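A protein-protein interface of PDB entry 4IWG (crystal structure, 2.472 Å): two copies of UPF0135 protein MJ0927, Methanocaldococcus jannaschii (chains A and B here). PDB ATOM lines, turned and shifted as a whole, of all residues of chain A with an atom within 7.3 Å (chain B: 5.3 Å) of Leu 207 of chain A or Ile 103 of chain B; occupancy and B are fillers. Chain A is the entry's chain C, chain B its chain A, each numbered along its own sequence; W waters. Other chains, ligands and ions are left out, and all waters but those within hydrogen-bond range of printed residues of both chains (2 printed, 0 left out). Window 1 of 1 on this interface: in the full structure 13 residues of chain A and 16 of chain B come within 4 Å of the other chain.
Water W2 lies within hydrogen-bond range of O of Glu 206 of chain A (2.4 Å), OD2 of Asp 110 of chain B (2.7 Å) and NH2 of Arg 131 of chain B (2.9 Å).
Water W1 bridges O of Lys 182 of chain A (3.0 Å) and N of Gly 128 of chain B (3.1 Å).
O of Ala 185 of chain A touches CD of Pro 123 of chain B, 3.3 Å away.
Glu 186 of chain A touches Pro 123 of chain B.
Leu 203 of chain A touches Leu 18 of chain B.
Leu 18 of chain B touches Glu 206 of chain A (CD2 to CG, 3.9 Å).
OE1 of Glu 206 of chain A touches CB of Cys 104 of chain B, at 3.5 Å.
CG2 of Ile 103 of chain B touches CD2 of Leu 207 of chain A, at 3.9 Å.
OD1 of Asn 127 of chain B sits at hydrogen-bond distance from N of Leu 129 of chain B (3.1 Å).
O of Leu 101 of chain B lies within hydrogen-bond range of SG of Cys 104 of chain B, 3.7 Å away.
The backbone carbonyl oxygen (O) of Ile 103 of chain B is in hydrogen-bond range of the guanidinium group (NH2) of Arg 131 of chain B, at 2.8 Å.
The backbone carbonyl oxygen (O) of Asn 100 of chain B sits close to the side-chain sulfur (SG) of Cys 104 of chain B (3.4 Å).
No position is printed for both chains.
Lys 160 of chain A touches none of the printed residues of chain B.
Of the printed residues of chain B, Ala 185 of chain A touches Pro 123.
Of chain B, only Ile 103 (3.9 Å) comes within 4 Å of Leu 207 of chain A.
Gly 208 of chain A touches none of the printed residues of chain B.
Of the printed residues of chain A, Leu 18 of chain B touches Lys 182, Leu 203 and Glu 206.
Of the printed residues of chain A, Ile 103 of chain B touches Leu 207 (3.9 Å).
The nearest residue of chain B that does not touch Leu 207 of chain A is Arg 131 of chain B (4.1 Å).
The nearest printed residue of chain A that does not touch Lys 105 of chain B is Glu 205 of chain A (4.1 Å).
O of Leu 18 of chain B sits at hydrogen-bond distance from NZ of Lys 182 of chain A, 3.0 Å away.
The side-chain amino group (NZ) of Lys 182 of chain A sits at hydrogen-bond distance from the backbone carbonyl oxygen (O) of Asn 127 of chain B.
The backbone NH of Lys 105 of chain B sits at hydrogen-bond distance from the side-chain carboxylate of Glu 206 of chain A, 2.7 Å away.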
ATOM      1  N   SER A 159       1.180  26.206   4.115  1.00  0.00           N
ATOM      2  CA  SER A 159       0.396  27.215   3.398  1.00  0.00           C
ATOM      3  C   SER A 159      -0.240  28.270   4.286  1.00  0.00           C
ATOM      4  O   SER A 159      -0.659  29.305   3.792  1.00  0.00           O
ATOM      5  CB  SER A 159      -0.715  26.548   2.582  1.00  0.00           C
ATOM      6  OG  SER A 159      -0.346  25.250   2.163  1.00  0.00           O
ATOM      7  N   LYS A 160      -0.321  28.005   5.586  1.00  0.00           N
ATOM      8  CA  LYS A 160      -1.032  28.877   6.522  1.00  0.00           C
ATOM      9  C   LYS A 160      -0.441  28.657   7.906  1.00  0.00           C
ATOM     10  O   LYS A 160       0.117  27.595   8.176  1.00  0.00           O
ATOM     11  CB  LYS A 160      -2.509  28.484   6.554  1.00  0.00           C
ATOM     12  CG  LYS A 160      -3.483  29.633   6.581  1.00  0.00           C
ATOM     13  CD  LYS A 160      -4.917  29.148   6.335  1.00  0.00           C
ATOM     14  CE  LYS A 160      -5.632  29.963   5.221  1.00  0.00           C
ATOM     15  NZ  LYS A 160      -6.933  29.342   4.791  1.00  0.00           N
ATOM     16  N   GLN A 178      -4.870  16.373  -6.910  1.00  0.00           N
ATOM     17  CA  GLN A 178      -5.431  17.712  -6.987  1.00  0.00           C
ATOM     18  C   GLN A 178      -6.869  17.781  -6.493  1.00  0.00           C
ATOM     19  O   GLN A 178      -7.224  18.679  -5.731  1.00  0.00           O
ATOM     20  CB  GLN A 178      -5.318  18.258  -8.407  1.00  0.00           C
ATOM     21  CG  GLN A 178      -4.076  19.101  -8.615  1.00  0.00           C
ATOM     22  CD  GLN A 178      -3.894  19.523 -10.058  1.00  0.00           C
ATOM     23  OE1 GLN A 178      -4.624  20.383 -10.569  1.00  0.00           O
ATOM     24  NE2 GLN A 178      -2.910  18.920 -10.729  1.00  0.00           N
ATOM     25  N   ILE A 181      -7.163  17.167  -2.620  1.00  0.00           N
ATOM     26  CA  ILE A 181      -6.752  18.374  -1.915  1.00  0.00           C
ATOM     27  C   ILE A 181      -7.846  19.453  -1.871  1.00  0.00           C
ATOM     28  O   ILE A 181      -8.087  20.051  -0.817  1.00  0.00           O
ATOM     29  CB  ILE A 181      -5.457  18.921  -2.523  1.00  0.00           C
ATOM     30  CG1 ILE A 181      -4.302  17.976  -2.166  1.00  0.00           C
ATOM     31  CG2 ILE A 181      -5.194  20.344  -2.076  1.00  0.00           C
ATOM     32  CD1 ILE A 181      -2.958  18.624  -2.136  1.00  0.00           C
ATOM     33  N   LYS A 182      -8.516  19.693  -2.998  1.00  0.00           N
ATOM     34  CA  LYS A 182      -9.603  20.666  -3.027  1.00  0.00           C
ATOM     35  C   LYS A 182     -10.721  20.233  -2.078  1.00  0.00           C
ATOM     36  O   LYS A 182     -11.253  21.043  -1.320  1.00  0.00           O
ATOM     37  CB  LYS A 182     -10.150  20.847  -4.447  1.00  0.00           C
ATOM     38  CG  LYS A 182      -9.207  21.566  -5.395  1.00  0.00           C
ATOM     39  CD  LYS A 182      -9.772  21.607  -6.816  1.00  0.00           C
ATOM     40  CE  LYS A 182      -9.443  22.950  -7.502  1.00  0.00           C
ATOM     41  NZ  LYS A 182      -9.983  23.118  -8.903  1.00  0.00           N
ATOM     42  N   TYR A 183     -11.059  18.952  -2.107  1.00  0.00           N
ATOM     43  CA  TYR A 183     -12.139  18.459  -1.272  1.00  0.00           C
ATOM     44  C   TYR A 183     -11.802  18.668   0.215  1.00  0.00           C
ATOM     45  O   TYR A 183     -12.559  19.289   0.956  1.00  0.00           O
ATOM     46  CB  TYR A 183     -12.428  16.986  -1.598  1.00  0.00           C
ATOM     47  CG  TYR A 183     -13.437  16.329  -0.690  1.00  0.00           C
ATOM     48  CD1 TYR A 183     -14.800  16.409  -0.950  1.00  0.00           C
ATOM     49  CD2 TYR A 183     -13.025  15.627   0.437  1.00  0.00           C
ATOM     50  CE1 TYR A 183     -15.729  15.806  -0.103  1.00  0.00           C
ATOM     51  CE2 TYR A 183     -13.936  15.025   1.284  1.00  0.00           C
ATOM     52  CZ  TYR A 183     -15.280  15.118   1.013  1.00  0.00           C
ATOM     53  OH  TYR A 183     -16.167  14.521   1.867  1.00  0.00           O
ATOM     54  N   VAL A 184     -10.640  18.181   0.627  1.00  0.00           N
ATOM     55  CA  VAL A 184     -10.228  18.239   2.016  1.00  0.00           C
ATOM     56  C   VAL A 184      -9.982  19.671   2.477  1.00  0.00           C
ATOM     57  O   VAL A 184     -10.129  19.983   3.655  1.00  0.00           O
ATOM     58  CB  VAL A 184      -8.982  17.381   2.241  1.00  0.00           C
ATOM     59  CG1 VAL A 184      -8.519  17.460   3.690  1.00  0.00           C
ATOM     60  CG2 VAL A 184      -9.271  15.938   1.834  1.00  0.00           C
ATOM     61  N   ALA A 185      -9.641  20.557   1.546  1.00  0.00           N
ATOM     62  CA  ALA A 185      -9.430  21.955   1.908  1.00  0.00           C
ATOM     63  C   ALA A 185     -10.710  22.593   2.469  1.00  0.00           C
ATOM     64  O   ALA A 185     -10.647  23.618   3.156  1.00  0.00           O
ATOM     65  CB  ALA A 185      -8.900  22.755   0.721  1.00  0.00           C
ATOM     66  N   GLU A 186     -11.862  21.988   2.182  1.00  0.00           N
ATOM     67  CA  GLU A 186     -13.141  22.470   2.717  1.00  0.00           C
ATOM     68  C   GLU A 186     -13.331  22.088   4.174  1.00  0.00           C
ATOM     69  O   GLU A 186     -14.119  22.705   4.879  1.00  0.00           O
ATOM     70  CB  GLU A 186     -14.320  21.831   1.984  1.00  0.00           C
ATOM     71  CG  GLU A 186     -14.477  22.162   0.537  1.00  0.00           C
ATOM     72  CD  GLU A 186     -15.576  21.329  -0.096  1.00  0.00           C
ATOM     73  OE1 GLU A 186     -16.756  21.703   0.042  1.00  0.00           O
ATOM     74  OE2 GLU A 186     -15.262  20.293  -0.722  1.00  0.00           O
ATOM     75  N   LYS A 201       1.129  20.649  -4.601  1.00  0.00           N
ATOM     76  CA  LYS A 201       1.775  21.548  -3.660  1.00  0.00           C
ATOM     77  C   LYS A 201       1.294  22.971  -3.895  1.00  0.00           C
ATOM     78  O   LYS A 201       0.871  23.653  -2.957  1.00  0.00           O
ATOM     79  CB  LYS A 201       3.303  21.455  -3.758  1.00  0.00           C
ATOM     80  CG  LYS A 201       4.066  22.629  -3.132  1.00  0.00           C
ATOM     81  CD  LYS A 201       5.568  22.339  -3.030  1.00  0.00           C
ATOM     82  CE  LYS A 201       6.365  23.551  -2.551  1.00  0.00           C
ATOM     83  NZ  LYS A 201       7.796  23.216  -2.221  1.00  0.00           N
ATOM     84  N   ILE A 202       1.338  23.414  -5.147  1.00  0.00           N
ATOM     85  CA  ILE A 202       0.881  24.767  -5.496  1.00  0.00           C
ATOM     86  C   ILE A 202      -0.597  24.978  -5.149  1.00  0.00           C
ATOM     87  O   ILE A 202      -0.965  25.986  -4.534  1.00  0.00           O
ATOM     88  CB  ILE A 202       1.095  25.073  -6.983  1.00  0.00           C
ATOM     89  CG1 ILE A 202       2.592  25.044  -7.318  1.00  0.00           C
ATOM     90  CG2 ILE A 202       0.498  26.430  -7.337  1.00  0.00           C
ATOM     91  CD1 ILE A 202       3.367  26.205  -6.724  1.00  0.00           C
ATOM     92  N   LEU A 203      -1.424  24.012  -5.535  1.00  0.00           N
ATOM     93  CA  LEU A 203      -2.836  24.020  -5.217  1.00  0.00           C
ATOM     94  C   LEU A 203      -3.075  24.215  -3.704  1.00  0.00           C
ATOM     95  O   LEU A 203      -3.848  25.095  -3.295  1.00  0.00           O
ATOM     96  CB  LEU A 203      -3.473  22.725  -5.703  1.00  0.00           C
ATOM     97  CG  LEU A 203      -4.952  22.552  -5.348  1.00  0.00           C
ATOM     98  CD1 LEU A 203      -5.787  23.644  -5.975  1.00  0.00           C
ATOM     99  CD2 LEU A 203      -5.442  21.177  -5.769  1.00  0.00           C
ATOM    100  N   ALA A 204      -2.394  23.407  -2.888  1.00  0.00           N
ATOM    101  CA  ALA A 204      -2.474  23.503  -1.429  1.00  0.00           C
ATOM    102  C   ALA A 204      -2.137  24.892  -0.923  1.00  0.00           C
ATOM    103  O   ALA A 204      -2.842  25.434  -0.075  1.00  0.00           O
ATOM    104  CB  ALA A 204      -1.566  22.476  -0.770  1.00  0.00           C
ATOM    105  N   GLU A 205      -1.061  25.473  -1.441  1.00  0.00           N
ATOM    106  CA  GLU A 205      -0.689  26.837  -1.048  1.00  0.00           C
ATOM    107  C   GLU A 205      -1.741  27.886  -1.417  1.00  0.00           C
ATOM    108  O   GLU A 205      -2.003  28.809  -0.639  1.00  0.00           O
ATOM    109  CB  GLU A 205       0.672  27.213  -1.629  1.00  0.00           C
ATOM    110  CG  GLU A 205       1.807  26.345  -1.111  1.00  0.00           C
ATOM    111  CD  GLU A 205       3.079  26.486  -1.928  1.00  0.00           C
ATOM    112  OE1 GLU A 205       3.185  27.462  -2.706  1.00  0.00           O
ATOM    113  OE2 GLU A 205       3.966  25.613  -1.806  1.00  0.00           O
ATOM    114  N   GLU A 206      -2.343  27.735  -2.599  1.00  0.00           N
ATOM    115  CA  GLU A 206      -3.392  28.636  -3.068  1.00  0.00           C
ATOM    116  C   GLU A 206      -4.644  28.579  -2.172  1.00  0.00           C
ATOM    117  O   GLU A 206      -5.269  29.614  -1.894  1.00  0.00           O
ATOM    118  CB  GLU A 206      -3.766  28.311  -4.522  1.00  0.00           C
ATOM    119  CG  GLU A 206      -2.619  28.477  -5.533  1.00  0.00           C
ATOM    120  CD  GLU A 206      -2.261  29.935  -5.829  1.00  0.00           C
ATOM    121  OE1 GLU A 206      -3.027  30.851  -5.459  1.00  0.00           O
ATOM    122  OE2 GLU A 206      -1.201  30.173  -6.445  1.00  0.00           O
ATOM    123  N   LEU A 207      -5.006  27.374  -1.722  1.00  0.00           N
ATOM    124  CA  LEU A 207      -6.220  27.179  -0.931  1.00  0.00           C
ATOM    125  C   LEU A 207      -5.980  27.395   0.554  1.00  0.00           C
ATOM    126  O   LEU A 207      -6.920  27.612   1.310  1.00  0.00           O
ATOM    127  CB  LEU A 207      -6.825  25.794  -1.170  1.00  0.00           C
ATOM    128  CG  LEU A 207      -7.164  25.499  -2.630  1.00  0.00           C
ATOM    129  CD1 LEU A 207      -7.864  24.139  -2.810  1.00  0.00           C
ATOM    130  CD2 LEU A 207      -7.967  26.646  -3.235  1.00  0.00           C
ATOM    131  N   GLY A 208      -4.720  27.337   0.972  1.00  0.00           N
ATOM    132  CA  GLY A 208      -4.389  27.533   2.365  1.00  0.00           C
ATOM    133  C   GLY A 208      -4.543  26.277   3.194  1.00  0.00           C
ATOM    134  O   GLY A 208      -4.708  26.348   4.410  1.00  0.00           O
ATOM    135  N   LEU A 209      -4.501  25.123   2.545  1.00  0.00           N
ATOM    136  CA  LEU A 209      -4.493  23.867   3.261  1.00  0.00           C
ATOM    137  C   LEU A 209      -3.048  23.438   3.553  1.00  0.00           C
ATOM    138  O   LEU A 209      -2.247  23.238   2.630  1.00  0.00           O
ATOM    139  CB  LEU A 209      -5.208  22.794   2.442  1.00  0.00           C
ATOM    140  CG  LEU A 209      -5.194  21.349   2.966  1.00  0.00           C
ATOM    141  CD1 LEU A 209      -5.908  21.223   4.338  1.00  0.00           C
ATOM    142  CD2 LEU A 209      -5.779  20.369   1.933  1.00  0.00           C
ATOM    143  N   VAL A 210      -2.718  23.287   4.833  1.00  0.00           N
ATOM    144  CA  VAL A 210      -1.403  22.771   5.226  1.00  0.00           C
ATOM    145  C   VAL A 210      -1.338  21.271   4.928  1.00  0.00           C
ATOM    146  O   VAL A 210      -2.206  20.500   5.344  1.00  0.00           O
ATOM    147  CB  VAL A 210      -1.101  23.041   6.725  1.00  0.00           C
ATOM    148  CG1 VAL A 210       0.207  22.372   7.148  1.00  0.00           C
ATOM    149  CG2 VAL A 210      -1.059  24.547   7.010  1.00  0.00           C
ATOM    150  N   LEU B  18      -5.882  25.422 -11.586  1.00  0.00           N
ATOM    151  CA  LEU B  18      -6.847  25.814 -10.577  1.00  0.00           C
ATOM    152  C   LEU B  18      -8.278  25.845 -11.144  1.00  0.00           C
ATOM    153  O   LEU B  18      -9.245  25.584 -10.423  1.00  0.00           O
ATOM    154  CB  LEU B  18      -6.458  27.167 -10.012  1.00  0.00           C
ATOM    155  CG  LEU B  18      -5.826  27.167  -8.622  1.00  0.00           C
ATOM    156  CD1 LEU B  18      -4.667  26.196  -8.532  1.00  0.00           C
ATOM    157  CD2 LEU B  18      -5.383  28.576  -8.300  1.00  0.00           C
ATOM    158  N   ALA B  19      -8.401  26.155 -12.435  1.00  0.00           N
ATOM    159  CA  ALA B  19      -9.690  26.201 -13.124  1.00  0.00           C
ATOM    160  C   ALA B  19     -10.537  24.925 -12.980  1.00  0.00           C
ATOM    161  O   ALA B  19     -10.013  23.814 -12.929  1.00  0.00           O
ATOM    162  CB  ALA B  19      -9.484  26.520 -14.598  1.00  0.00           C
ATOM    163  N   ILE B  20     -11.852  25.093 -12.909  1.00  0.00           N
ATOM    164  CA  ILE B  20     -12.737  23.947 -12.782  1.00  0.00           C
ATOM    165  C   ILE B  20     -12.766  23.196 -14.094  1.00  0.00           C
ATOM    166  O   ILE B  20     -12.379  23.726 -15.144  1.00  0.00           O
ATOM    167  CB  ILE B  20     -14.183  24.349 -12.388  1.00  0.00           C
ATOM    168  CG1 ILE B  20     -14.889  25.062 -13.548  1.00  0.00           C
ATOM    169  CG2 ILE B  20     -14.177  25.204 -11.136  1.00  0.00           C
ATOM    170  CD1 ILE B  20     -16.348  25.404 -13.264  1.00  0.00           C
ATOM    171  N   THR B  99     -12.177  30.864 -13.820  1.00  0.00           N
ATOM    172  CA  THR B  99     -12.254  30.294 -12.472  1.00  0.00           C
ATOM    173  C   THR B  99     -10.884  30.213 -11.772  1.00  0.00           C
ATOM    174  O   THR B  99     -10.817  30.233 -10.551  1.00  0.00           O
ATOM    175  CB  THR B  99     -12.982  28.936 -12.431  1.00  0.00           C
ATOM    176  OG1 THR B  99     -12.309  27.999 -13.282  1.00  0.00           O
ATOM    177  CG2 THR B  99     -14.422  29.093 -12.893  1.00  0.00           C
ATOM    178  N   ASN B 100      -9.792  30.150 -12.528  1.00  0.00           N
ATOM    179  CA  ASN B 100      -8.479  30.200 -11.886  1.00  0.00           C
ATOM    180  C   ASN B 100      -8.250  31.527 -11.143  1.00  0.00           C
ATOM    181  O   ASN B 100      -7.663  31.555 -10.071  1.00  0.00           O
ATOM    182  CB  ASN B 100      -7.308  29.793 -12.824  1.00  0.00           C
ATOM    183  CG  ASN B 100      -7.301  30.535 -14.171  1.00  0.00           C
ATOM    184  OD1 ASN B 100      -8.335  30.787 -14.780  1.00  0.00           O
ATOM    185  ND2 ASN B 100      -6.114  30.851 -14.644  1.00  0.00           N
ATOM    186  N   LEU B 101      -8.765  32.619 -11.684  1.00  0.00           N
ATOM    187  CA  LEU B 101      -8.705  33.891 -10.970  1.00  0.00           C
ATOM    188  C   LEU B 101      -9.723  33.927  -9.817  1.00  0.00           C
ATOM    189  O   LEU B 101      -9.587  34.698  -8.876  1.00  0.00           O
ATOM    190  CB  LEU B 101      -8.942  35.050 -11.932  1.00  0.00           C
ATOM    191  CG  LEU B 101      -8.694  36.433 -11.337  1.00  0.00           C
ATOM    192  CD1 LEU B 101      -7.255  36.538 -10.809  1.00  0.00           C
ATOM    193  CD2 LEU B 101      -8.983  37.507 -12.359  1.00  0.00           C
ATOM    194  N   ASP B 102     -10.740  33.078  -9.889  1.00  0.00           N
ATOM    195  CA  ASP B 102     -11.741  32.993  -8.839  1.00  0.00           C
ATOM    196  C   ASP B 102     -11.169  32.227  -7.656  1.00  0.00           C
ATOM    197  O   ASP B 102     -11.421  32.567  -6.497  1.00  0.00           O
ATOM    198  CB  ASP B 102     -12.987  32.253  -9.344  1.00  0.00           C
ATOM    199  CG  ASP B 102     -13.821  33.076 -10.316  1.00  0.00           C
ATOM    200  OD1 ASP B 102     -14.165  34.224 -10.003  1.00  0.00           O
ATOM    201  OD2 ASP B 102     -14.154  32.570 -11.403  1.00  0.00           O
ATOM    202  N   ILE B 103     -10.388  31.194  -7.961  1.00  0.00           N
ATOM    203  CA  ILE B 103      -9.947  30.214  -6.970  1.00  0.00           C
ATOM    204  C   ILE B 103      -8.580  30.517  -6.319  1.00  0.00           C
ATOM    205  O   ILE B 103      -8.326  30.128  -5.180  1.00  0.00           O
ATOM    206  CB  ILE B 103      -9.959  28.805  -7.604  1.00  0.00           C
ATOM    207  CG1 ILE B 103     -11.380  28.471  -8.047  1.00  0.00           C
ATOM    208  CG2 ILE B 103      -9.417  27.757  -6.649  1.00  0.00           C
ATOM    209  CD1 ILE B 103     -11.516  27.196  -8.785  1.00  0.00           C
ATOM    210  N   CYS B 104      -7.714  31.232  -7.028  1.00  0.00           N
ATOM    211  CA  CYS B 104      -6.354  31.473  -6.552  1.00  0.00           C
ATOM    212  C   CYS B 104      -6.308  32.327  -5.281  1.00  0.00           C
ATOM    213  O   CYS B 104      -7.250  33.073  -4.968  1.00  0.00           O
ATOM    214  CB  CYS B 104      -5.512  32.129  -7.648  1.00  0.00           C
ATOM    215  SG  CYS B 104      -6.043  33.798  -8.057  1.00  0.00           S
ATOM    216  N   LYS B 105      -5.201  32.207  -4.554  1.00  0.00           N
ATOM    217  CA  LYS B 105      -4.985  32.998  -3.355  1.00  0.00           C
ATOM    218  C   LYS B 105      -5.020  34.480  -3.716  1.00  0.00           C
ATOM    219  O   LYS B 105      -4.362  34.913  -4.668  1.00  0.00           O
ATOM    220  CB  LYS B 105      -3.655  32.627  -2.717  1.00  0.00           C
ATOM    221  CG  LYS B 105      -3.377  33.309  -1.381  1.00  0.00           C
ATOM    222  CD  LYS B 105      -2.016  32.878  -0.861  1.00  0.00           C
ATOM    223  CE  LYS B 105      -1.628  33.625   0.400  1.00  0.00           C
ATOM    224  NZ  LYS B 105      -0.258  33.210   0.832  1.00  0.00           N
ATOM    225  N   ASN B 109     -12.747  35.327  -5.082  1.00  0.00           N
ATOM    226  CA  ASN B 109     -13.402  34.850  -3.872  1.00  0.00           C
ATOM    227  C   ASN B 109     -12.672  35.232  -2.575  1.00  0.00           C
ATOM    228  O   ASN B 109     -13.313  35.658  -1.620  1.00  0.00           O
ATOM    229  CB  ASN B 109     -13.677  33.348  -3.968  1.00  0.00           C
ATOM    230  CG  ASN B 109     -14.821  33.029  -4.929  1.00  0.00           C
ATOM    231  OD1 ASN B 109     -15.963  33.432  -4.692  1.00  0.00           O
ATOM    232  ND2 ASN B 109     -14.522  32.308  -6.012  1.00  0.00           N
ATOM    233  N   ASP B 110     -11.344  35.105  -2.552  1.00  0.00           N
ATOM    234  CA  ASP B 110     -10.546  35.523  -1.389  1.00  0.00           C
ATOM    235  C   ASP B 110     -10.739  37.008  -1.076  1.00  0.00           C
ATOM    236  O   ASP B 110     -10.832  37.393   0.077  1.00  0.00           O
ATOM    237  CB  ASP B 110      -9.051  35.256  -1.614  1.00  0.00           C
ATOM    238  CG  ASP B 110      -8.604  33.892  -1.101  1.00  0.00           C
ATOM    239  OD1 ASP B 110      -9.414  33.171  -0.468  1.00  0.00           O
ATOM    240  OD2 ASP B 110      -7.418  33.548  -1.326  1.00  0.00           O
ATOM    241  N   PRO B 123     -12.519  26.994   1.304  1.00  0.00           N
ATOM    242  CA  PRO B 123     -13.267  26.956   0.040  1.00  0.00           C
ATOM    243  C   PRO B 123     -14.668  26.388   0.269  1.00  0.00           C
ATOM    244  O   PRO B 123     -14.860  25.579   1.170  1.00  0.00           O
ATOM    245  CB  PRO B 123     -12.430  26.017  -0.841  1.00  0.00           C
ATOM    246  CG  PRO B 123     -11.070  26.002  -0.223  1.00  0.00           C
ATOM    247  CD  PRO B 123     -11.283  26.189   1.247  1.00  0.00           C
ATOM    248  N   ASN B 127     -14.801  22.109  -6.048  1.00  0.00           N
ATOM    249  CA  ASN B 127     -13.927  22.523  -7.143  1.00  0.00           C
ATOM    250  C   ASN B 127     -13.070  23.755  -6.822  1.00  0.00           C
ATOM    251  O   ASN B 127     -12.400  24.309  -7.702  1.00  0.00           O
ATOM    252  CB  ASN B 127     -14.760  22.773  -8.406  1.00  0.00           C
ATOM    253  CG  ASN B 127     -15.883  23.776  -8.170  1.00  0.00           C
ATOM    254  OD1 ASN B 127     -15.854  24.552  -7.206  1.00  0.00           O
ATOM    255  ND2 ASN B 127     -16.872  23.771  -9.053  1.00  0.00           N
ATOM    256  N   GLY B 128     -13.086  24.178  -5.563  1.00  0.00           N
ATOM    257  CA  GLY B 128     -12.263  25.292  -5.143  1.00  0.00           C
ATOM    258  C   GLY B 128     -12.979  26.628  -5.087  1.00  0.00           C
ATOM    259  O   GLY B 128     -12.420  27.592  -4.561  1.00  0.00           O
ATOM    260  N   LEU B 129     -14.202  26.702  -5.620  1.00  0.00           N
ATOM    261  CA  LEU B 129     -14.926  27.979  -5.681  1.00  0.00           C
ATOM    262  C   LEU B 129     -15.563  28.453  -4.368  1.00  0.00           C
ATOM    263  O   LEU B 129     -16.005  27.665  -3.538  1.00  0.00           O
ATOM    264  CB  LEU B 129     -15.990  27.946  -6.773  1.00  0.00           C
ATOM    265  CG  LEU B 129     -15.459  28.006  -8.209  1.00  0.00           C
ATOM    266  CD1 LEU B 129     -16.585  27.739  -9.173  1.00  0.00           C
ATOM    267  CD2 LEU B 129     -14.852  29.348  -8.489  1.00  0.00           C
ATOM    268  N   ARG B 131     -15.884  30.978  -0.750  1.00  0.00           N
ATOM    269  CA  ARG B 131     -15.252  30.914   0.560  1.00  0.00           C
ATOM    270  C   ARG B 131     -16.357  30.925   1.603  1.00  0.00           C
ATOM    271  O   ARG B 131     -17.420  31.502   1.384  1.00  0.00           O
ATOM    272  CB  ARG B 131     -14.293  32.099   0.749  1.00  0.00           C
ATOM    273  CG  ARG B 131     -13.070  32.109  -0.215  1.00  0.00           C
ATOM    274  CD  ARG B 131     -12.154  30.881  -0.003  1.00  0.00           C
ATOM    275  NE  ARG B 131     -10.953  30.887  -0.843  1.00  0.00           N
ATOM    276  CZ  ARG B 131     -10.840  30.246  -2.010  1.00  0.00           C
ATOM    277  NH1 ARG B 131     -11.854  29.550  -2.500  1.00  0.00           N
ATOM    278  NH2 ARG B 131      -9.706  30.297  -2.694  1.00  0.00           N
HETATM  279  O   HOH W   1     -12.411  23.449  -2.668  1.00  0.00           O
HETATM  280  O   HOH W   2      -7.234  30.891  -1.262  1.00  0.00           O
